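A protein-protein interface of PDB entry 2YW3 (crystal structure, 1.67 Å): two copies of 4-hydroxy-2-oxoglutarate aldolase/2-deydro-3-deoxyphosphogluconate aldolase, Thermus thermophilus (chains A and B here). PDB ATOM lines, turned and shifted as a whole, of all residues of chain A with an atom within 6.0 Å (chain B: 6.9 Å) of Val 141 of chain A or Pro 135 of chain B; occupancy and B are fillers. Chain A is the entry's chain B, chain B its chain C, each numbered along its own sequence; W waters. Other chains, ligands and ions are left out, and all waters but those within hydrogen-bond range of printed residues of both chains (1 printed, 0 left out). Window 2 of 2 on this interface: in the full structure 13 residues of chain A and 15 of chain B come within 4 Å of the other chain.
The guanidinium group (NH2) of Arg 140 of chain A sits at hydrogen-bond distance from the backbone carbonyl oxygen (O) of Glu 134 of chain B.
The backbone NH (N) of Glu 134 of chain B lies within hydrogen-bond range of the backbone carbonyl oxygen (O) of Gly 158 of chain B (2.9 Å).
Among the printed residues, merely in contact across the chains: Phe 136 of chain A with Phe 136 of chain B, Gln 137 of chain A with Pro 135 of chain B, Arg 140 of chain A with Pro 135 of chain B, Val 141 of chain A with Pro 135 of chain B and Val 141 of chain A with Phe 136 of chain B.
Val 141 of chain A touches just these residues of chain B: Pro 135 and Phe 136.
Pro 135 of chain B touches just these residues of chain A: Gln 137 (3.3 Å), Arg 140 (3.5 Å) and Val 141 (3.7 Å).
Of the printed residues of chain A, Glu 134 of chain B touches Arg 140 (3.4 Å).
Printed residues of chain B within 4 Å of Gln 137 of chain A: Pro 135 (3.3 Å).
Of the printed residues of chain A, Phe 136 of chain B touches Phe 136 and Val 141.
Printed residues of chain B within 4 Å of Arg 140 of chain A: Glu 134 and Pro 135.
The nearest residue of chain B that does not touch Val 141 of chain A is Pro 132 of chain B (4.6 Å).
The nearest printed residue of chain B that does not touch Gln 137 of chain A is Phe 136 of chain B (5.5 Å).
Of the 13 printed residues of chain B, 3 touch a printed residue of chain A.
Hydrophobic or aromatic side chains of chain B within 4 Å of the printed part of chain A: Pro 135 and Phe 136.
Hydrophobic or aromatic side chains of chain A within 4 Å of the printed part of chain B: Phe 136 and Val 141.
Among the printed residues, 6 pairs touch across the chains.
Among the printed residues, no Asp or Glu carboxylate lies within 4 Å of a Lys or Arg side-chain nitrogen of the other chain.
Phe 136 of chain A touches its own counterpart, Phe 136 of chain B.
Water W1 bridges the backbone carbonyl oxygen of Pro 135 of chain B and the backbone carbonyl oxygen of Phe 136 of chain A.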
ATOM      1  N   LEU A 112       0.674 -35.248  32.321  1.00  0.00           N
ATOM      2  CA  LEU A 112      -0.093 -34.229  31.591  1.00  0.00           C
ATOM      3  C   LEU A 112      -1.545 -34.641  31.369  1.00  0.00           C
ATOM      4  O   LEU A 112      -2.466 -33.839  31.567  1.00  0.00           O
ATOM      5  CB  LEU A 112       0.535 -33.971  30.230  1.00  0.00           C
ATOM      6  CG  LEU A 112       1.790 -33.114  30.226  1.00  0.00           C
ATOM      7  CD1 LEU A 112       2.430 -33.219  28.859  1.00  0.00           C
ATOM      8  CD2 LEU A 112       1.443 -31.603  30.586  1.00  0.00           C
ATOM      9  N   PHE A 130       2.749 -31.184  37.105  1.00  0.00           N
ATOM     10  CA  PHE A 130       2.085 -31.041  35.809  1.00  0.00           C
ATOM     11  C   PHE A 130       3.129 -30.344  34.951  1.00  0.00           C
ATOM     12  O   PHE A 130       3.453 -29.194  35.198  1.00  0.00           O
ATOM     13  CB  PHE A 130       0.814 -30.182  35.919  1.00  0.00           C
ATOM     14  CG  PHE A 130       0.082 -30.029  34.610  1.00  0.00           C
ATOM     15  CD1 PHE A 130      -0.786 -31.029  34.162  1.00  0.00           C
ATOM     16  CD2 PHE A 130       0.270 -28.884  33.809  1.00  0.00           C
ATOM     17  CE1 PHE A 130      -1.453 -30.913  32.946  1.00  0.00           C
ATOM     18  CE2 PHE A 130      -0.425 -28.749  32.587  1.00  0.00           C
ATOM     19  CZ  PHE A 130      -1.273 -29.781  32.145  1.00  0.00           C
ATOM     20  N   PHE A 136       1.393 -26.604  27.718  1.00  0.00           N
ATOM     21  CA  PHE A 136       0.187 -27.433  27.662  1.00  0.00           C
ATOM     22  C   PHE A 136      -1.046 -26.822  28.349  1.00  0.00           C
ATOM     23  O   PHE A 136      -1.877 -27.563  28.897  1.00  0.00           O
ATOM     24  CB  PHE A 136       0.475 -28.844  28.184  1.00  0.00           C
ATOM     25  CG  PHE A 136       1.216 -29.722  27.209  1.00  0.00           C
ATOM     26  CD1 PHE A 136       0.531 -30.397  26.198  1.00  0.00           C
ATOM     27  CD2 PHE A 136       2.580 -29.908  27.327  1.00  0.00           C
ATOM     28  CE1 PHE A 136       1.217 -31.241  25.295  1.00  0.00           C
ATOM     29  CE2 PHE A 136       3.269 -30.751  26.440  1.00  0.00           C
ATOM     30  CZ  PHE A 136       2.581 -31.413  25.423  1.00  0.00           C
ATOM     31  N   GLN A 137      -1.173 -25.489  28.293  1.00  0.00           N
ATOM     32  CA  GLN A 137      -2.331 -24.748  28.830  1.00  0.00           C
ATOM     33  C   GLN A 137      -2.662 -25.058  30.302  1.00  0.00           C
ATOM     34  O   GLN A 137      -3.815 -25.330  30.664  1.00  0.00           O
ATOM     35  CB  GLN A 137      -3.578 -24.931  27.930  1.00  0.00           C
ATOM     36  CG  GLN A 137      -3.441 -24.295  26.526  1.00  0.00           C
ATOM     37  CD  GLN A 137      -3.482 -22.772  26.561  1.00  0.00           C
ATOM     38  OE1 GLN A 137      -3.986 -22.161  27.519  1.00  0.00           O
ATOM     39  NE2 GLN A 137      -2.950 -22.149  25.515  1.00  0.00           N
ATOM     40  N   GLY A 138      -1.636 -24.991  31.140  1.00  0.00           N
ATOM     41  CA  GLY A 138      -1.715 -25.351  32.542  1.00  0.00           C
ATOM     42  C   GLY A 138      -2.929 -24.904  33.320  1.00  0.00           C
ATOM     43  O   GLY A 138      -3.565 -25.723  33.978  1.00  0.00           O
ATOM     44  N   VAL A 139      -3.258 -23.608  33.294  1.00  0.00           N
ATOM     45  CA  VAL A 139      -4.328 -23.133  34.195  1.00  0.00           C
ATOM     46  C   VAL A 139      -5.664 -23.766  33.790  1.00  0.00           C
ATOM     47  O   VAL A 139      -6.441 -24.245  34.632  1.00  0.00           O
ATOM     48  CB  VAL A 139      -4.429 -21.578  34.206  1.00  0.00           C
ATOM     49  CG1 VAL A 139      -5.739 -21.134  34.924  1.00  0.00           C
ATOM     50  CG2 VAL A 139      -3.187 -20.997  34.900  1.00  0.00           C
ATOM     51  N   ARG A 140      -5.898 -23.838  32.491  1.00  0.00           N
ATOM     52  CA  ARG A 140      -7.191 -24.323  32.025  1.00  0.00           C
ATOM     53  C   ARG A 140      -7.317 -25.845  32.159  1.00  0.00           C
ATOM     54  O   ARG A 140      -8.392 -26.360  32.513  1.00  0.00           O
ATOM     55  CB  ARG A 140      -7.401 -23.908  30.590  1.00  0.00           C
ATOM     56  CG  ARG A 140      -7.603 -22.412  30.449  1.00  0.00           C
ATOM     57  CD  ARG A 140      -7.432 -22.069  29.021  1.00  0.00           C
ATOM     58  NE  ARG A 140      -8.488 -22.684  28.241  1.00  0.00           N
ATOM     59  CZ  ARG A 140      -8.407 -22.911  26.937  1.00  0.00           C
ATOM     60  NH1 ARG A 140      -7.298 -22.594  26.277  1.00  0.00           N
ATOM     61  NH2 ARG A 140      -9.428 -23.463  26.303  1.00  0.00           N
ATOM     62  N   VAL A 141      -6.209 -26.540  31.940  1.00  0.00           N
ATOM     63  CA  VAL A 141      -6.194 -27.999  32.173  1.00  0.00           C
ATOM     64  C   VAL A 141      -6.402 -28.277  33.659  1.00  0.00           C
ATOM     65  O   VAL A 141      -7.250 -29.084  34.023  1.00  0.00           O
ATOM     66  CB  VAL A 141      -4.894 -28.632  31.713  1.00  0.00           C
ATOM     67  CG1 VAL A 141      -4.913 -30.122  32.024  1.00  0.00           C
ATOM     68  CG2 VAL A 141      -4.694 -28.409  30.223  1.00  0.00           C
ATOM     69  N   LEU A 142      -5.641 -27.604  34.524  1.00  0.00           N
ATOM     70  CA  LEU A 142      -5.802 -27.848  35.949  1.00  0.00           C
ATOM     71  C   LEU A 142      -7.162 -27.485  36.498  1.00  0.00           C
ATOM     72  O   LEU A 142      -7.620 -28.106  37.469  1.00  0.00           O
ATOM     73  CB  LEU A 142      -4.698 -27.168  36.742  1.00  0.00           C
ATOM     74  CG  LEU A 142      -3.303 -27.707  36.436  1.00  0.00           C
ATOM     75  CD1 LEU A 142      -2.327 -26.989  37.354  1.00  0.00           C
ATOM     76  CD2 LEU A 142      -3.207 -29.240  36.671  1.00  0.00           C
ATOM     77  N   ARG A 143      -7.796 -26.477  35.896  1.00  0.00           N
ATOM     78  CA  ARG A 143      -9.158 -26.135  36.263  1.00  0.00           C
ATOM     79  C   ARG A 143     -10.098 -27.318  35.955  1.00  0.00           C
ATOM     80  O   ARG A 143     -10.957 -27.677  36.771  1.00  0.00           O
ATOM     81  CB  ARG A 143      -9.628 -24.862  35.563  1.00  0.00           C
ATOM     82  CG  ARG A 143     -11.094 -24.508  35.903  1.00  0.00           C
ATOM     83  CD  ARG A 143     -11.409 -23.007  35.854  1.00  0.00           C
ATOM     84  NE  ARG A 143     -10.841 -22.339  34.687  1.00  0.00           N
ATOM     85  CZ  ARG A 143      -9.934 -21.364  34.744  1.00  0.00           C
ATOM     86  NH1 ARG A 143      -9.494 -20.922  35.925  1.00  0.00           N
ATOM     87  NH2 ARG A 143      -9.474 -20.830  33.615  1.00  0.00           N
ATOM     88  N   ALA A 144      -9.903 -27.963  34.807  1.00  0.00           N
ATOM     89  CA  ALA A 144     -10.739 -29.134  34.479  1.00  0.00           C
ATOM     90  C   ALA A 144     -10.430 -30.282  35.454  1.00  0.00           C
ATOM     91  O   ALA A 144     -11.333 -30.990  35.929  1.00  0.00           O
ATOM     92  CB  ALA A 144     -10.518 -29.566  33.021  1.00  0.00           C
ATOM     93  N   TYR A 145      -9.156 -30.437  35.809  1.00  0.00           N
ATOM     94  CA  TYR A 145      -8.772 -31.561  36.678  1.00  0.00           C
ATOM     95  C   TYR A 145      -9.268 -31.371  38.104  1.00  0.00           C
ATOM     96  O   TYR A 145      -9.467 -32.353  38.813  1.00  0.00           O
ATOM     97  CB  TYR A 145      -7.262 -31.778  36.678  1.00  0.00           C
ATOM     98  CG  TYR A 145      -6.717 -32.298  35.374  1.00  0.00           C
ATOM     99  CD1 TYR A 145      -7.564 -32.568  34.276  1.00  0.00           C
ATOM    100  CD2 TYR A 145      -5.353 -32.534  35.231  1.00  0.00           C
ATOM    101  CE1 TYR A 145      -7.044 -33.065  33.070  1.00  0.00           C
ATOM    102  CE2 TYR A 145      -4.814 -33.047  34.014  1.00  0.00           C
ATOM    103  CZ  TYR A 145      -5.670 -33.300  32.955  1.00  0.00           C
ATOM    104  OH  TYR A 145      -5.150 -33.773  31.767  1.00  0.00           O
ATOM    105  N   ALA A 146      -9.493 -30.112  38.504  1.00  0.00           N
ATOM    106  CA  ALA A 146      -9.979 -29.817  39.844  1.00  0.00           C
ATOM    107  C   ALA A 146     -11.336 -30.467  40.069  1.00  0.00           C
ATOM    108  O   ALA A 146     -11.599 -30.930  41.171  1.00  0.00           O
ATOM    109  CB  ALA A 146     -10.075 -28.287  40.093  1.00  0.00           C
ATOM    110  N   LEU B 112      -6.264 -38.330  24.815  1.00  0.00           N
ATOM    111  CA  LEU B 112      -5.729 -37.083  24.244  1.00  0.00           C
ATOM    112  C   LEU B 112      -4.709 -37.361  23.123  1.00  0.00           C
ATOM    113  O   LEU B 112      -4.786 -36.764  22.039  1.00  0.00           O
ATOM    114  CB  LEU B 112      -5.118 -36.190  25.324  1.00  0.00           C
ATOM    115  CG  LEU B 112      -6.113 -35.417  26.187  1.00  0.00           C
ATOM    116  CD1 LEU B 112      -5.425 -34.714  27.324  1.00  0.00           C
ATOM    117  CD2 LEU B 112      -6.836 -34.387  25.280  1.00  0.00           C
ATOM    118  N   PHE B 131     -10.658 -35.431  25.796  1.00  0.00           N
ATOM    119  CA  PHE B 131     -10.894 -34.689  27.026  1.00  0.00           C
ATOM    120  C   PHE B 131      -9.593 -34.388  27.737  1.00  0.00           C
ATOM    121  O   PHE B 131      -8.749 -35.283  27.863  1.00  0.00           O
ATOM    122  CB  PHE B 131     -11.802 -35.453  28.004  1.00  0.00           C
ATOM    123  CG  PHE B 131     -11.846 -34.819  29.388  1.00  0.00           C
ATOM    124  CD1 PHE B 131     -12.728 -33.763  29.654  1.00  0.00           C
ATOM    125  CD2 PHE B 131     -10.961 -35.229  30.400  1.00  0.00           C
ATOM    126  CE1 PHE B 131     -12.758 -33.134  30.930  1.00  0.00           C
ATOM    127  CE2 PHE B 131     -10.984 -34.616  31.677  1.00  0.00           C
ATOM    128  CZ  PHE B 131     -11.882 -33.556  31.930  1.00  0.00           C
ATOM    129  N   PRO B 132      -9.428 -33.137  28.224  1.00  0.00           N
ATOM    130  CA  PRO B 132     -10.331 -31.945  28.042  1.00  0.00           C
ATOM    131  C   PRO B 132     -10.060 -31.238  26.716  1.00  0.00           C
ATOM    132  O   PRO B 132      -8.940 -30.845  26.434  1.00  0.00           O
ATOM    133  CB  PRO B 132      -9.982 -31.036  29.223  1.00  0.00           C
ATOM    134  CG  PRO B 132      -8.570 -31.490  29.679  1.00  0.00           C
ATOM    135  CD  PRO B 132      -8.265 -32.852  29.092  1.00  0.00           C
ATOM    136  N   ALA B 133     -11.118 -31.058  25.941  1.00  0.00           N
ATOM    137  CA  ALA B 133     -10.995 -30.746  24.539  1.00  0.00           C
ATOM    138  C   ALA B 133     -10.467 -29.337  24.283  1.00  0.00           C
ATOM    139  O   ALA B 133      -9.492 -29.154  23.540  1.00  0.00           O
ATOM    140  CB  ALA B 133     -12.360 -30.961  23.860  1.00  0.00           C
ATOM    141  N   GLU B 134     -11.115 -28.339  24.890  1.00  0.00           N
ATOM    142  CA  GLU B 134     -10.719 -26.961  24.562  1.00  0.00           C
ATOM    143  C   GLU B 134      -9.300 -26.604  25.042  1.00  0.00           C
ATOM    144  O   GLU B 134      -8.530 -26.012  24.277  1.00  0.00           O
ATOM    145  CB  GLU B 134     -11.776 -25.956  25.009  1.00  0.00           C
ATOM    146  CG  GLU B 134     -12.917 -25.851  24.012  1.00  0.00           C
ATOM    147  CD  GLU B 134     -12.445 -25.586  22.584  1.00  0.00           C
ATOM    148  OE1 GLU B 134     -11.791 -24.550  22.343  1.00  0.00           O
ATOM    149  OE2 GLU B 134     -12.720 -26.414  21.702  1.00  0.00           O
ATOM    150  N   PRO B 135      -8.935 -26.952  26.293  1.00  0.00           N
ATOM    151  CA  PRO B 135      -7.549 -26.675  26.681  1.00  0.00           C
ATOM    152  C   PRO B 135      -6.478 -27.356  25.828  1.00  0.00           C
ATOM    153  O   PRO B 135      -5.372 -26.814  25.715  1.00  0.00           O
ATOM    154  CB  PRO B 135      -7.485 -27.212  28.107  1.00  0.00           C
ATOM    155  CG  PRO B 135      -8.851 -26.999  28.602  1.00  0.00           C
ATOM    156  CD  PRO B 135      -9.682 -27.491  27.432  1.00  0.00           C
ATOM    157  N   PHE B 136      -6.789 -28.517  25.250  1.00  0.00           N
ATOM    158  CA  PHE B 136      -5.816 -29.214  24.385  1.00  0.00           C
ATOM    159  C   PHE B 136      -6.112 -29.035  22.880  1.00  0.00           C
ATOM    160  O   PHE B 136      -5.850 -29.938  22.073  1.00  0.00           O
ATOM    161  CB  PHE B 136      -5.750 -30.695  24.747  1.00  0.00           C
ATOM    162  CG  PHE B 136      -5.015 -30.991  26.028  1.00  0.00           C
ATOM    163  CD1 PHE B 136      -3.627 -31.162  26.036  1.00  0.00           C
ATOM    164  CD2 PHE B 136      -5.706 -31.177  27.208  1.00  0.00           C
ATOM    165  CE1 PHE B 136      -2.923 -31.459  27.243  1.00  0.00           C
ATOM    166  CE2 PHE B 136      -5.029 -31.484  28.401  1.00  0.00           C
ATOM    167  CZ  PHE B 136      -3.636 -31.631  28.419  1.00  0.00           C
ATOM    168  N   GLN B 137      -6.659 -27.875  22.508  1.00  0.00           N
ATOM    169  CA  GLN B 137      -6.825 -27.509  21.096  1.00  0.00           C
ATOM    170  C   GLN B 137      -7.619 -28.519  20.277  1.00  0.00           C
ATOM    171  O   GLN B 137      -7.222 -28.915  19.166  1.00  0.00           O
ATOM    172  CB  GLN B 137      -5.448 -27.269  20.475  1.00  0.00           C
ATOM    173  CG  GLN B 137      -4.696 -26.133  21.162  1.00  0.00           C
ATOM    174  CD  GLN B 137      -4.772 -24.879  20.352  1.00  0.00           C
ATOM    175  OE1 GLN B 137      -5.854 -24.335  20.122  1.00  0.00           O
ATOM    176  NE2 GLN B 137      -3.623 -24.420  19.877  1.00  0.00           N
ATOM    177  N   GLY B 138      -8.763 -28.918  20.829  1.00  0.00           N
ATOM    178  CA  GLY B 138      -9.596 -29.941  20.224  1.00  0.00           C
ATOM    179  C   GLY B 138      -9.824 -29.897  18.727  1.00  0.00           C
ATOM    180  O   GLY B 138      -9.668 -30.902  18.060  1.00  0.00           O
ATOM    181  N   THR B 157     -15.086 -33.122  24.745  1.00  0.00           N
ATOM    182  CA  THR B 157     -15.759 -32.585  25.917  1.00  0.00           C
ATOM    183  C   THR B 157     -14.712 -31.861  26.728  1.00  0.00           C
ATOM    184  O   THR B 157     -13.559 -32.307  26.799  1.00  0.00           O
ATOM    185  CB  THR B 157     -16.324 -33.748  26.790  1.00  0.00           C
ATOM    186  OG1 THR B 157     -17.244 -34.522  25.999  1.00  0.00           O
ATOM    187  CG2 THR B 157     -17.024 -33.219  28.049  1.00  0.00           C
ATOM    188  N   GLY B 158     -15.087 -30.738  27.328  1.00  0.00           N
ATOM    189  CA  GLY B 158     -14.181 -30.020  28.215  1.00  0.00           C
ATOM    190  C   GLY B 158     -14.002 -28.581  27.773  1.00  0.00           C
ATOM    191  O   GLY B 158     -13.216 -28.286  26.865  1.00  0.00           O
ATOM    192  N   GLY B 159     -14.738 -27.681  28.420  1.00  0.00           N
ATOM    193  CA  GLY B 159     -14.613 -26.247  28.068  1.00  0.00           C
ATOM    194  C   GLY B 159     -15.247 -25.832  26.747  1.00  0.00           C
ATOM    195  O   GLY B 159     -14.987 -24.731  26.250  1.00  0.00           O
ATOM    196  N   ILE B 160     -16.103 -26.673  26.180  1.00  0.00           N
ATOM    197  CA  ILE B 160     -16.765 -26.320  24.939  1.00  0.00           C
ATOM    198  C   ILE B 160     -17.889 -25.309  25.212  1.00  0.00           C
ATOM    199  O   ILE B 160     -18.609 -25.414  26.199  1.00  0.00           O
ATOM    200  CB  ILE B 160     -17.247 -27.552  24.202  1.00  0.00           C
ATOM    201  CG1 ILE B 160     -16.003 -28.428  23.857  1.00  0.00           C
ATOM    202  CG2 ILE B 160     -17.920 -27.159  22.911  1.00  0.00           C
ATOM    203  CD1 ILE B 160     -16.319 -29.651  23.062  1.00  0.00           C
HETATM  204  O   HOH W   1      -2.752 -27.995  25.757  1.00  0.00           O
